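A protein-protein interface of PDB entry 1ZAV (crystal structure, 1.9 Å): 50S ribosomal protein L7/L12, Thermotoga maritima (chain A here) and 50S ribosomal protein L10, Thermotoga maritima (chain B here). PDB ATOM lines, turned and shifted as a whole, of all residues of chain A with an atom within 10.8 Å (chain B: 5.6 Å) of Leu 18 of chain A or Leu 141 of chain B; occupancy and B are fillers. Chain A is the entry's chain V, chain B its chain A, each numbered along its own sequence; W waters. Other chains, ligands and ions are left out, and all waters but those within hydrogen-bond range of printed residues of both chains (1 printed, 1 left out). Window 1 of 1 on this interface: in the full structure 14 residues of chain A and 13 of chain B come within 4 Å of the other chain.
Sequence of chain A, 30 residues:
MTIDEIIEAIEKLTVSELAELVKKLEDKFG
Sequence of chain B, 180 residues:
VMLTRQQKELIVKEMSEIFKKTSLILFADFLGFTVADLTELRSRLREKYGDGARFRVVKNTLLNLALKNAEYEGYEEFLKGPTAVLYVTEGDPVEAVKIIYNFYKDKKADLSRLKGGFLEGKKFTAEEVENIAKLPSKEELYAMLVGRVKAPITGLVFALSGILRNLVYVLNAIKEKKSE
Ala 9 of chain A touches none of the printed residues of chain B. Printed residues of chain B within 4 Å of Ile 10 of chain A: Leu 145 (3.5 Å). Ser 16 of chain A touches none of the printed residues of chain B. Of chain B, only Lys 138, Leu 141 and Tyr 142 come within 4 Å of Leu 18 of chain A. Printed residues of chain B within 4 Å of Leu 21 of chain A: Leu 145 (3.8 Å). No residue of chain A comes within 4 Å of Pro 136 of chain B. No residue of chain A comes within 4 Å of Glu 140 of chain B. Leu 141 of chain B touches two residues of chain A. Tyr 142 of chain B touches just these residues of chain A: Glu 11 and Leu 18. No residue of chain A comes within 4 Å of Ala 143 of chain B. No residue of chain A comes within 4 Å of Met 144 of chain B. Of the printed residues of chain A, Leu 145 of chain B touches Ile 10 (3.5 Å), Leu 21 (3.8 Å) and Leu 25 (3.6 Å). The nearest printed residue of chain A that does not touch Leu 141 of chain B is Val 22 of chain A (4.1 Å).
Printed residues of chain B that touch a printed residue of chain A: Lys 138, Leu 141, Tyr 142 and Leu 145. Hydrophobic or aromatic side chains of chain B that line the printed part of chain A: Leu 141, Tyr 142 and Leu 145. Along chain B the printed residues that touch a printed residue of chain A span positions 138 to 145. Among the printed residues, 10 pairs touch across the chains. Among the printed residues, no Asp or Glu carboxylate lies within 4 Å of a Lys or Arg side-chain nitrogen of the other chain.
The side-chain amino group of Lys 138 of chain B sits at hydrogen-bond distance from the backbone carbonyl oxygen of Leu 13 of chain A, at 2.8 Å. The side-chain hydroxyl (OH) of Tyr 142 of chain B is in hydrogen-bond range of the backbone carbonyl oxygen (O) of Glu 11 of chain A, at 3.4 Å.
Leu 145 of chain B touches Ile 10 of chain A (CD2 to CG2, 3.5 Å). Lys 138 of chain B touches Val 15 of chain A. Val 15 of chain A touches Leu 141 of chain B. Lys 138 of chain B touches Leu 18 of chain A. CD2 of Leu 18 of chain A touches CB of Leu 141 of chain B, at 3.1 Å. CE2 of Tyr 142 of chain B touches CD1 of Leu 18 of chain A, 3.4 Å away. Leu 145 of chain B touches Leu 21 of chain A. CD1 of Leu 145 of chain B touches CD2 of Leu 25 of chain A (3.6 Å).
Water W1 lies within hydrogen-bond range of O of Glu 11 of chain A, NZ of Lys 138 of chain B and O of Leu 13 of chain A.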
ATOM      1  N   ILE A   6       9.649 -15.876 -17.073  1.00  0.00           N
ATOM      2  CA  ILE A   6      10.322 -14.767 -16.406  1.00  0.00           C
ATOM      3  C   ILE A   6       9.909 -13.455 -17.059  1.00  0.00           C
ATOM      4  O   ILE A   6       9.481 -12.516 -16.384  1.00  0.00           O
ATOM      5  CB  ILE A   6      11.862 -14.869 -16.514  1.00  0.00           C
ATOM      6  CG1 ILE A   6      12.360 -16.138 -15.829  1.00  0.00           C
ATOM      7  CG2 ILE A   6      12.505 -13.649 -15.874  1.00  0.00           C
ATOM      8  CD1 ILE A   6      13.855 -16.344 -15.975  1.00  0.00           C
ATOM      9  N   ILE A   7      10.048 -13.397 -18.380  1.00  0.00           N
ATOM     10  CA  ILE A   7       9.714 -12.198 -19.135  1.00  0.00           C
ATOM     11  C   ILE A   7       8.263 -11.780 -18.922  1.00  0.00           C
ATOM     12  O   ILE A   7       7.960 -10.589 -18.807  1.00  0.00           O
ATOM     13  CB  ILE A   7       9.961 -12.415 -20.643  1.00  0.00           C
ATOM     14  CG1 ILE A   7      11.450 -12.688 -20.886  1.00  0.00           C
ATOM     15  CG2 ILE A   7       9.505 -11.185 -21.428  1.00  0.00           C
ATOM     16  CD1 ILE A   7      11.774 -13.172 -22.280  1.00  0.00           C
ATOM     17  N   GLU A   8       7.371 -12.764 -18.860  1.00  0.00           N
ATOM     18  CA  GLU A   8       5.952 -12.487 -18.667  1.00  0.00           C
ATOM     19  C   GLU A   8       5.694 -11.862 -17.304  1.00  0.00           C
ATOM     20  O   GLU A   8       4.969 -10.875 -17.199  1.00  0.00           O
ATOM     21  CB  GLU A   8       5.138 -13.769 -18.835  1.00  0.00           C
ATOM     22  CG  GLU A   8       5.191 -14.317 -20.253  1.00  0.00           C
ATOM     23  CD  GLU A   8       4.374 -15.581 -20.433  1.00  0.00           C
ATOM     24  OE1 GLU A   8       4.354 -16.116 -21.565  1.00  0.00           O
ATOM     25  OE2 GLU A   8       3.754 -16.041 -19.446  1.00  0.00           O
ATOM     26  N   ALA A   9       6.299 -12.430 -16.263  1.00  0.00           N
ATOM     27  CA  ALA A   9       6.140 -11.899 -14.914  1.00  0.00           C
ATOM     28  C   ALA A   9       6.708 -10.481 -14.851  1.00  0.00           C
ATOM     29  O   ALA A   9       6.169  -9.610 -14.170  1.00  0.00           O
ATOM     30  CB  ALA A   9       6.855 -12.794 -13.909  1.00  0.00           C
ATOM     31  N   ILE A  10       7.798 -10.251 -15.573  1.00  0.00           N
ATOM     32  CA  ILE A  10       8.434  -8.941 -15.586  1.00  0.00           C
ATOM     33  C   ILE A  10       7.571  -7.844 -16.198  1.00  0.00           C
ATOM     34  O   ILE A  10       7.472  -6.746 -15.652  1.00  0.00           O
ATOM     35  CB  ILE A  10       9.782  -8.996 -16.333  1.00  0.00           C
ATOM     36  CG1 ILE A  10      10.827  -9.672 -15.441  1.00  0.00           C
ATOM     37  CG2 ILE A  10      10.233  -7.590 -16.735  1.00  0.00           C
ATOM     38  CD1 ILE A  10      12.138  -9.976 -16.140  1.00  0.00           C
ATOM     39  N   GLU A  11       6.951  -8.135 -17.334  1.00  0.00           N
ATOM     40  CA  GLU A  11       6.123  -7.142 -18.007  1.00  0.00           C
ATOM     41  C   GLU A  11       4.795  -6.860 -17.298  1.00  0.00           C
ATOM     42  O   GLU A  11       4.061  -5.954 -17.688  1.00  0.00           O
ATOM     43  CB  GLU A  11       5.886  -7.563 -19.461  1.00  0.00           C
ATOM     44  CG  GLU A  11       5.466  -9.008 -19.632  1.00  0.00           C
ATOM     45  CD  GLU A  11       5.488  -9.451 -21.086  1.00  0.00           C
ATOM     46  OE1 GLU A  11       6.579  -9.444 -21.701  1.00  0.00           O
ATOM     47  OE2 GLU A  11       4.414  -9.806 -21.617  1.00  0.00           O
ATOM     48  N   LYS A  12       4.492  -7.625 -16.253  1.00  0.00           N
ATOM     49  CA  LYS A  12       3.263  -7.420 -15.492  1.00  0.00           C
ATOM     50  C   LYS A  12       3.504  -6.562 -14.250  1.00  0.00           C
ATOM     51  O   LYS A  12       2.559  -6.178 -13.556  1.00  0.00           O
ATOM     52  CB  LYS A  12       2.669  -8.762 -15.064  1.00  0.00           C
ATOM     53  CG  LYS A  12       2.157  -9.596 -16.218  1.00  0.00           C
ATOM     54  CD  LYS A  12       1.584 -10.920 -15.739  1.00  0.00           C
ATOM     55  CE  LYS A  12       1.055 -11.729 -16.913  1.00  0.00           C
ATOM     56  NZ  LYS A  12       0.045 -10.948 -17.688  1.00  0.00           N
ATOM     57  N   LEU A  13       4.770  -6.261 -13.969  1.00  0.00           N
ATOM     58  CA  LEU A  13       5.119  -5.460 -12.801  1.00  0.00           C
ATOM     59  C   LEU A  13       4.716  -3.999 -12.951  1.00  0.00           C
ATOM     60  O   LEU A  13       4.719  -3.452 -14.057  1.00  0.00           O
ATOM     61  CB  LEU A  13       6.630  -5.522 -12.536  1.00  0.00           C
ATOM     62  CG  LEU A  13       7.301  -6.846 -12.164  1.00  0.00           C
ATOM     63  CD1 LEU A  13       8.774  -6.566 -11.933  1.00  0.00           C
ATOM     64  CD2 LEU A  13       6.671  -7.460 -10.914  1.00  0.00           C
ATOM     65  N   THR A  14       4.374  -3.367 -11.832  1.00  0.00           N
ATOM     66  CA  THR A  14       4.008  -1.953 -11.858  1.00  0.00           C
ATOM     67  C   THR A  14       5.323  -1.191 -11.987  1.00  0.00           C
ATOM     68  O   THR A  14       6.390  -1.799 -12.010  1.00  0.00           O
ATOM     69  CB  THR A  14       3.325  -1.507 -10.553  1.00  0.00           C
ATOM     70  OG1 THR A  14       4.270  -1.589  -9.476  1.00  0.00           O
ATOM     71  CG2 THR A  14       2.121  -2.392 -10.243  1.00  0.00           C
ATOM     72  N   VAL A  15       5.252   0.133 -12.071  1.00  0.00           N
ATOM     73  CA  VAL A  15       6.463   0.934 -12.184  1.00  0.00           C
ATOM     74  C   VAL A  15       7.297   0.800 -10.906  1.00  0.00           C
ATOM     75  O   VAL A  15       8.522   0.659 -10.961  1.00  0.00           O
ATOM     76  CB  VAL A  15       6.122   2.416 -12.410  1.00  0.00           C
ATOM     77  CG1 VAL A  15       7.384   3.275 -12.269  1.00  0.00           C
ATOM     78  CG2 VAL A  15       5.491   2.592 -13.790  1.00  0.00           C
ATOM     79  N   SER A  16       6.626   0.839  -9.759  1.00  0.00           N
ATOM     80  CA  SER A  16       7.310   0.726  -8.478  1.00  0.00           C
ATOM     81  C   SER A  16       7.986  -0.633  -8.316  1.00  0.00           C
ATOM     82  O   SER A  16       9.134  -0.715  -7.885  1.00  0.00           O
ATOM     83  CB  SER A  16       6.324   0.972  -7.334  1.00  0.00           C
ATOM     84  OG  SER A  16       6.928   0.724  -6.077  1.00  0.00           O
ATOM     85  N   GLU A  17       7.272  -1.697  -8.671  1.00  0.00           N
ATOM     86  CA  GLU A  17       7.793  -3.050  -8.570  1.00  0.00           C
ATOM     87  C   GLU A  17       8.978  -3.257  -9.501  1.00  0.00           C
ATOM     88  O   GLU A  17       9.965  -3.899  -9.131  1.00  0.00           O
ATOM     89  CB  GLU A  17       6.693  -4.061  -8.909  1.00  0.00           C
ATOM     90  CG  GLU A  17       5.611  -4.165  -7.840  1.00  0.00           C
ATOM     91  CD  GLU A  17       4.407  -4.974  -8.291  1.00  0.00           C
ATOM     92  OE1 GLU A  17       3.526  -5.242  -7.446  1.00  0.00           O
ATOM     93  OE2 GLU A  17       4.331  -5.335  -9.482  1.00  0.00           O
ATOM     94  N   LEU A  18       8.867  -2.715 -10.710  1.00  0.00           N
ATOM     95  CA  LEU A  18       9.918  -2.827 -11.714  1.00  0.00           C
ATOM     96  C   LEU A  18      11.182  -2.109 -11.243  1.00  0.00           C
ATOM     97  O   LEU A  18      12.291  -2.595 -11.458  1.00  0.00           O
ATOM     98  CB  LEU A  18       9.436  -2.221 -13.041  1.00  0.00           C
ATOM     99  CG  LEU A  18      10.250  -2.408 -14.327  1.00  0.00           C
ATOM    100  CD1 LEU A  18       9.472  -1.846 -15.513  1.00  0.00           C
ATOM    101  CD2 LEU A  18      11.583  -1.718 -14.203  1.00  0.00           C
ATOM    102  N   ALA A  19      11.006  -0.950 -10.614  1.00  0.00           N
ATOM    103  CA  ALA A  19      12.131  -0.161 -10.111  1.00  0.00           C
ATOM    104  C   ALA A  19      12.839  -0.927  -8.996  1.00  0.00           C
ATOM    105  O   ALA A  19      14.071  -0.900  -8.890  1.00  0.00           O
ATOM    106  CB  ALA A  19      11.639   1.191  -9.591  1.00  0.00           C
ATOM    107  N   GLU A  20      12.048  -1.609  -8.170  1.00  0.00           N
ATOM    108  CA  GLU A  20      12.585  -2.400  -7.078  1.00  0.00           C
ATOM    109  C   GLU A  20      13.409  -3.548  -7.677  1.00  0.00           C
ATOM    110  O   GLU A  20      14.498  -3.868  -7.180  1.00  0.00           O
ATOM    111  CB  GLU A  20      11.443  -2.951  -6.212  1.00  0.00           C
ATOM    112  CG  GLU A  20      11.910  -3.628  -4.928  1.00  0.00           C
ATOM    113  CD  GLU A  20      10.792  -4.330  -4.183  1.00  0.00           C
ATOM    114  OE1 GLU A  20       9.799  -3.664  -3.820  1.00  0.00           O
ATOM    115  OE2 GLU A  20      10.908  -5.553  -3.954  1.00  0.00           O
ATOM    116  N   LEU A  21      12.889  -4.159  -8.745  1.00  0.00           N
ATOM    117  CA  LEU A  21      13.573  -5.260  -9.428  1.00  0.00           C
ATOM    118  C   LEU A  21      14.926  -4.815  -9.977  1.00  0.00           C
ATOM    119  O   LEU A  21      15.942  -5.504  -9.817  1.00  0.00           O
ATOM    120  CB  LEU A  21      12.724  -5.787 -10.593  1.00  0.00           C
ATOM    121  CG  LEU A  21      13.387  -6.872 -11.461  1.00  0.00           C
ATOM    122  CD1 LEU A  21      13.642  -8.122 -10.626  1.00  0.00           C
ATOM    123  CD2 LEU A  21      12.499  -7.207 -12.657  1.00  0.00           C
ATOM    124  N   VAL A  22      14.928  -3.670 -10.646  1.00  0.00           N
ATOM    125  CA  VAL A  22      16.151  -3.139 -11.223  1.00  0.00           C
ATOM    126  C   VAL A  22      17.186  -2.868 -10.136  1.00  0.00           C
ATOM    127  O   VAL A  22      18.358  -3.211 -10.291  1.00  0.00           O
ATOM    128  CB  VAL A  22      15.861  -1.848 -12.009  1.00  0.00           C
ATOM    129  CG1 VAL A  22      17.162  -1.188 -12.464  1.00  0.00           C
ATOM    130  CG2 VAL A  22      14.996  -2.184 -13.216  1.00  0.00           C
ATOM    131  N   LYS A  23      16.754  -2.270  -9.031  1.00  0.00           N
ATOM    132  CA  LYS A  23      17.680  -1.965  -7.946  1.00  0.00           C
ATOM    133  C   LYS A  23      18.235  -3.212  -7.261  1.00  0.00           C
ATOM    134  O   LYS A  23      19.419  -3.261  -6.923  1.00  0.00           O
ATOM    135  CB  LYS A  23      17.013  -1.037  -6.925  1.00  0.00           C
ATOM    136  CG  LYS A  23      16.581   0.294  -7.532  1.00  0.00           C
ATOM    137  CD  LYS A  23      16.105   1.280  -6.485  1.00  0.00           C
ATOM    138  CE  LYS A  23      15.531   2.540  -7.128  1.00  0.00           C
ATOM    139  NZ  LYS A  23      16.500   3.248  -8.032  1.00  0.00           N
ATOM    140  N   LYS A  24      17.397  -4.223  -7.054  1.00  0.00           N
ATOM    141  CA  LYS A  24      17.882  -5.445  -6.427  1.00  0.00           C
ATOM    142  C   LYS A  24      18.858  -6.171  -7.366  1.00  0.00           C
ATOM    143  O   LYS A  24      19.858  -6.738  -6.930  1.00  0.00           O
ATOM    144  CB  LYS A  24      16.703  -6.357  -6.050  1.00  0.00           C
ATOM    145  CG  LYS A  24      15.948  -5.878  -4.811  1.00  0.00           C
ATOM    146  CD  LYS A  24      14.885  -6.874  -4.356  1.00  0.00           C
ATOM    147  CE  LYS A  24      14.270  -6.434  -3.029  1.00  0.00           C
ATOM    148  NZ  LYS A  24      13.099  -7.283  -2.644  1.00  0.00           N
ATOM    149  N   LEU A  25      18.566  -6.148  -8.660  1.00  0.00           N
ATOM    150  CA  LEU A  25      19.435  -6.789  -9.638  1.00  0.00           C
ATOM    151  C   LEU A  25      20.775  -6.050  -9.614  1.00  0.00           C
ATOM    152  O   LEU A  25      21.849  -6.646  -9.703  1.00  0.00           O
ATOM    153  CB  LEU A  25      18.794  -6.686 -11.026  1.00  0.00           C
ATOM    154  CG  LEU A  25      18.315  -7.967 -11.712  1.00  0.00           C
ATOM    155  CD1 LEU A  25      17.976  -9.042 -10.698  1.00  0.00           C
ATOM    156  CD2 LEU A  25      17.119  -7.641 -12.590  1.00  0.00           C
ATOM    157  N   GLU A  26      20.675  -4.737  -9.472  1.00  0.00           N
ATOM    158  CA  GLU A  26      21.826  -3.843  -9.424  1.00  0.00           C
ATOM    159  C   GLU A  26      22.723  -4.213  -8.240  1.00  0.00           C
ATOM    160  O   GLU A  26      23.945  -4.259  -8.374  1.00  0.00           O
ATOM    161  CB  GLU A  26      21.310  -2.407  -9.288  1.00  0.00           C
ATOM    162  CG  GLU A  26      22.066  -1.340 -10.052  1.00  0.00           C
ATOM    163  CD  GLU A  26      21.239  -0.069 -10.218  1.00  0.00           C
ATOM    164  OE1 GLU A  26      20.267  -0.084 -11.005  1.00  0.00           O
ATOM    165  OE2 GLU A  26      21.553   0.947  -9.561  1.00  0.00           O
ATOM    166  N   PRO B 136      12.572   6.838 -12.787  1.00  0.00           N
ATOM    167  CA  PRO B 136      12.521   7.058 -14.237  1.00  0.00           C
ATOM    168  C   PRO B 136      11.245   6.447 -14.812  1.00  0.00           C
ATOM    169  O   PRO B 136      10.552   5.696 -14.127  1.00  0.00           O
ATOM    170  CB  PRO B 136      13.782   6.357 -14.733  1.00  0.00           C
ATOM    171  CG  PRO B 136      13.919   5.212 -13.774  1.00  0.00           C
ATOM    172  CD  PRO B 136      13.604   5.846 -12.436  1.00  0.00           C
ATOM    173  N   SER B 137      10.933   6.763 -16.062  1.00  0.00           N
ATOM    174  CA  SER B 137       9.727   6.224 -16.689  1.00  0.00           C
ATOM    175  C   SER B 137       9.826   4.712 -16.830  1.00  0.00           C
ATOM    176  O   SER B 137      10.919   4.151 -16.849  1.00  0.00           O
ATOM    177  CB  SER B 137       9.513   6.839 -18.073  1.00  0.00           C
ATOM    178  OG  SER B 137      10.498   6.387 -18.985  1.00  0.00           O
ATOM    179  N   LYS B 138       8.675   4.057 -16.936  1.00  0.00           N
ATOM    180  CA  LYS B 138       8.635   2.611 -17.079  1.00  0.00           C
ATOM    181  C   LYS B 138       9.481   2.186 -18.279  1.00  0.00           C
ATOM    182  O   LYS B 138      10.181   1.170 -18.232  1.00  0.00           O
ATOM    183  CB  LYS B 138       7.191   2.139 -17.259  1.00  0.00           C
ATOM    184  CG  LYS B 138       7.030   0.645 -17.111  1.00  0.00           C
ATOM    185  CD  LYS B 138       5.584   0.249 -16.909  1.00  0.00           C
ATOM    186  CE  LYS B 138       5.497  -1.205 -16.469  1.00  0.00           C
ATOM    187  NZ  LYS B 138       4.127  -1.602 -16.051  1.00  0.00           N
ATOM    188  N   GLU B 139       9.421   2.968 -19.352  1.00  0.00           N
ATOM    189  CA  GLU B 139      10.199   2.650 -20.540  1.00  0.00           C
ATOM    190  C   GLU B 139      11.691   2.688 -20.247  1.00  0.00           C
ATOM    191  O   GLU B 139      12.423   1.783 -20.642  1.00  0.00           O
ATOM    192  CB  GLU B 139       9.857   3.605 -21.687  1.00  0.00           C
ATOM    193  CG  GLU B 139       8.551   3.260 -22.383  1.00  0.00           C
ATOM    194  CD  GLU B 139       8.497   1.803 -22.840  1.00  0.00           C
ATOM    195  OE1 GLU B 139       9.376   1.382 -23.628  1.00  0.00           O
ATOM    196  OE2 GLU B 139       7.574   1.075 -22.408  1.00  0.00           O
ATOM    197  N   GLU B 140      12.138   3.732 -19.555  1.00  0.00           N
ATOM    198  CA  GLU B 140      13.547   3.861 -19.199  1.00  0.00           C
ATOM    199  C   GLU B 140      13.926   2.683 -18.297  1.00  0.00           C
ATOM    200  O   GLU B 140      15.017   2.119 -18.405  1.00  0.00           O
ATOM    201  CB  GLU B 140      13.790   5.185 -18.466  1.00  0.00           C
ATOM    202  CG  GLU B 140      13.417   6.415 -19.280  1.00  0.00           C
ATOM    203  CD  GLU B 140      13.637   7.722 -18.529  1.00  0.00           C
ATOM    204  OE1 GLU B 140      13.143   7.857 -17.389  1.00  0.00           O
ATOM    205  OE2 GLU B 140      14.297   8.626 -19.087  1.00  0.00           O
ATOM    206  N   LEU B 141      13.006   2.306 -17.418  1.00  0.00           N
ATOM    207  CA  LEU B 141      13.240   1.190 -16.509  1.00  0.00           C
ATOM    208  C   LEU B 141      13.449  -0.103 -17.281  1.00  0.00           C
ATOM    209  O   LEU B 141      14.407  -0.839 -17.020  1.00  0.00           O
ATOM    210  CB  LEU B 141      12.068   1.041 -15.540  1.00  0.00           C
ATOM    211  CG  LEU B 141      11.975   2.095 -14.436  1.00  0.00           C
ATOM    212  CD1 LEU B 141      10.651   1.943 -13.699  1.00  0.00           C
ATOM    213  CD2 LEU B 141      13.152   1.940 -13.473  1.00  0.00           C
ATOM    214  N   TYR B 142      12.560  -0.383 -18.231  1.00  0.00           N
ATOM    215  CA  TYR B 142      12.678  -1.591 -19.037  1.00  0.00           C
ATOM    216  C   TYR B 142      14.025  -1.594 -19.754  1.00  0.00           C
ATOM    217  O   TYR B 142      14.678  -2.630 -19.863  1.00  0.00           O
ATOM    218  CB  TYR B 142      11.547  -1.661 -20.068  1.00  0.00           C
ATOM    219  CG  TYR B 142      10.236  -2.199 -19.534  1.00  0.00           C
ATOM    220  CD1 TYR B 142       9.026  -1.600 -19.879  1.00  0.00           C
ATOM    221  CD2 TYR B 142      10.199  -3.328 -18.713  1.00  0.00           C
ATOM    222  CE1 TYR B 142       7.813  -2.105 -19.425  1.00  0.00           C
ATOM    223  CE2 TYR B 142       8.987  -3.848 -18.253  1.00  0.00           C
ATOM    224  CZ  TYR B 142       7.801  -3.228 -18.614  1.00  0.00           C
ATOM    225  OH  TYR B 142       6.603  -3.732 -18.167  1.00  0.00           O
ATOM    226  N   ALA B 143      14.430  -0.424 -20.241  1.00  0.00           N
ATOM    227  CA  ALA B 143      15.699  -0.282 -20.937  1.00  0.00           C
ATOM    228  C   ALA B 143      16.863  -0.681 -20.031  1.00  0.00           C
ATOM    229  O   ALA B 143      17.736  -1.442 -20.439  1.00  0.00           O
ATOM    230  CB  ALA B 143      15.879   1.157 -21.410  1.00  0.00           C
ATOM    231  N   MET B 144      16.867  -0.163 -18.804  1.00  0.00           N
ATOM    232  CA  MET B 144      17.925  -0.456 -17.838  1.00  0.00           C
ATOM    233  C   MET B 144      17.957  -1.922 -17.413  1.00  0.00           C
ATOM    234  O   MET B 144      19.019  -2.466 -17.106  1.00  0.00           O
ATOM    235  CB  MET B 144      17.748   0.390 -16.578  1.00  0.00           C
ATOM    236  CG  MET B 144      17.505   1.860 -16.812  1.00  0.00           C
ATOM    237  SD  MET B 144      17.099   2.691 -15.266  1.00  0.00           S
ATOM    238  CE  MET B 144      17.998   4.245 -15.445  1.00  0.00           C
ATOM    239  N   LEU B 145      16.787  -2.548 -17.374  1.00  0.00           N
ATOM    240  CA  LEU B 145      16.673  -3.941 -16.962  1.00  0.00           C
ATOM    241  C   LEU B 145      17.585  -4.873 -17.748  1.00  0.00           C
ATOM    242  O   LEU B 145      18.183  -5.788 -17.183  1.00  0.00           O
ATOM    243  CB  LEU B 145      15.222  -4.417 -17.099  1.00  0.00           C
ATOM    244  CG  LEU B 145      14.895  -5.793 -16.506  1.00  0.00           C
ATOM    245  CD1 LEU B 145      15.141  -5.782 -15.000  1.00  0.00           C
ATOM    246  CD2 LEU B 145      13.445  -6.143 -16.802  1.00  0.00           C
ATOM    247  N   VAL B 146      17.695  -4.639 -19.052  1.00  0.00           N
ATOM    248  CA  VAL B 146      18.530  -5.481 -19.899  1.00  0.00           C
ATOM    249  C   VAL B 146      19.992  -5.520 -19.449  1.00  0.00           C
ATOM    250  O   VAL B 146      20.577  -6.594 -19.351  1.00  0.00           O
ATOM    251  CB  VAL B 146      18.480  -5.027 -21.378  1.00  0.00           C
ATOM    252  CG1 VAL B 146      19.191  -3.695 -21.550  1.00  0.00           C
ATOM    253  CG2 VAL B 146      19.108  -6.087 -22.262  1.00  0.00           C
HETATM  254  O   HOH W   1       2.641  -3.877 -16.610  1.00  0.00           O
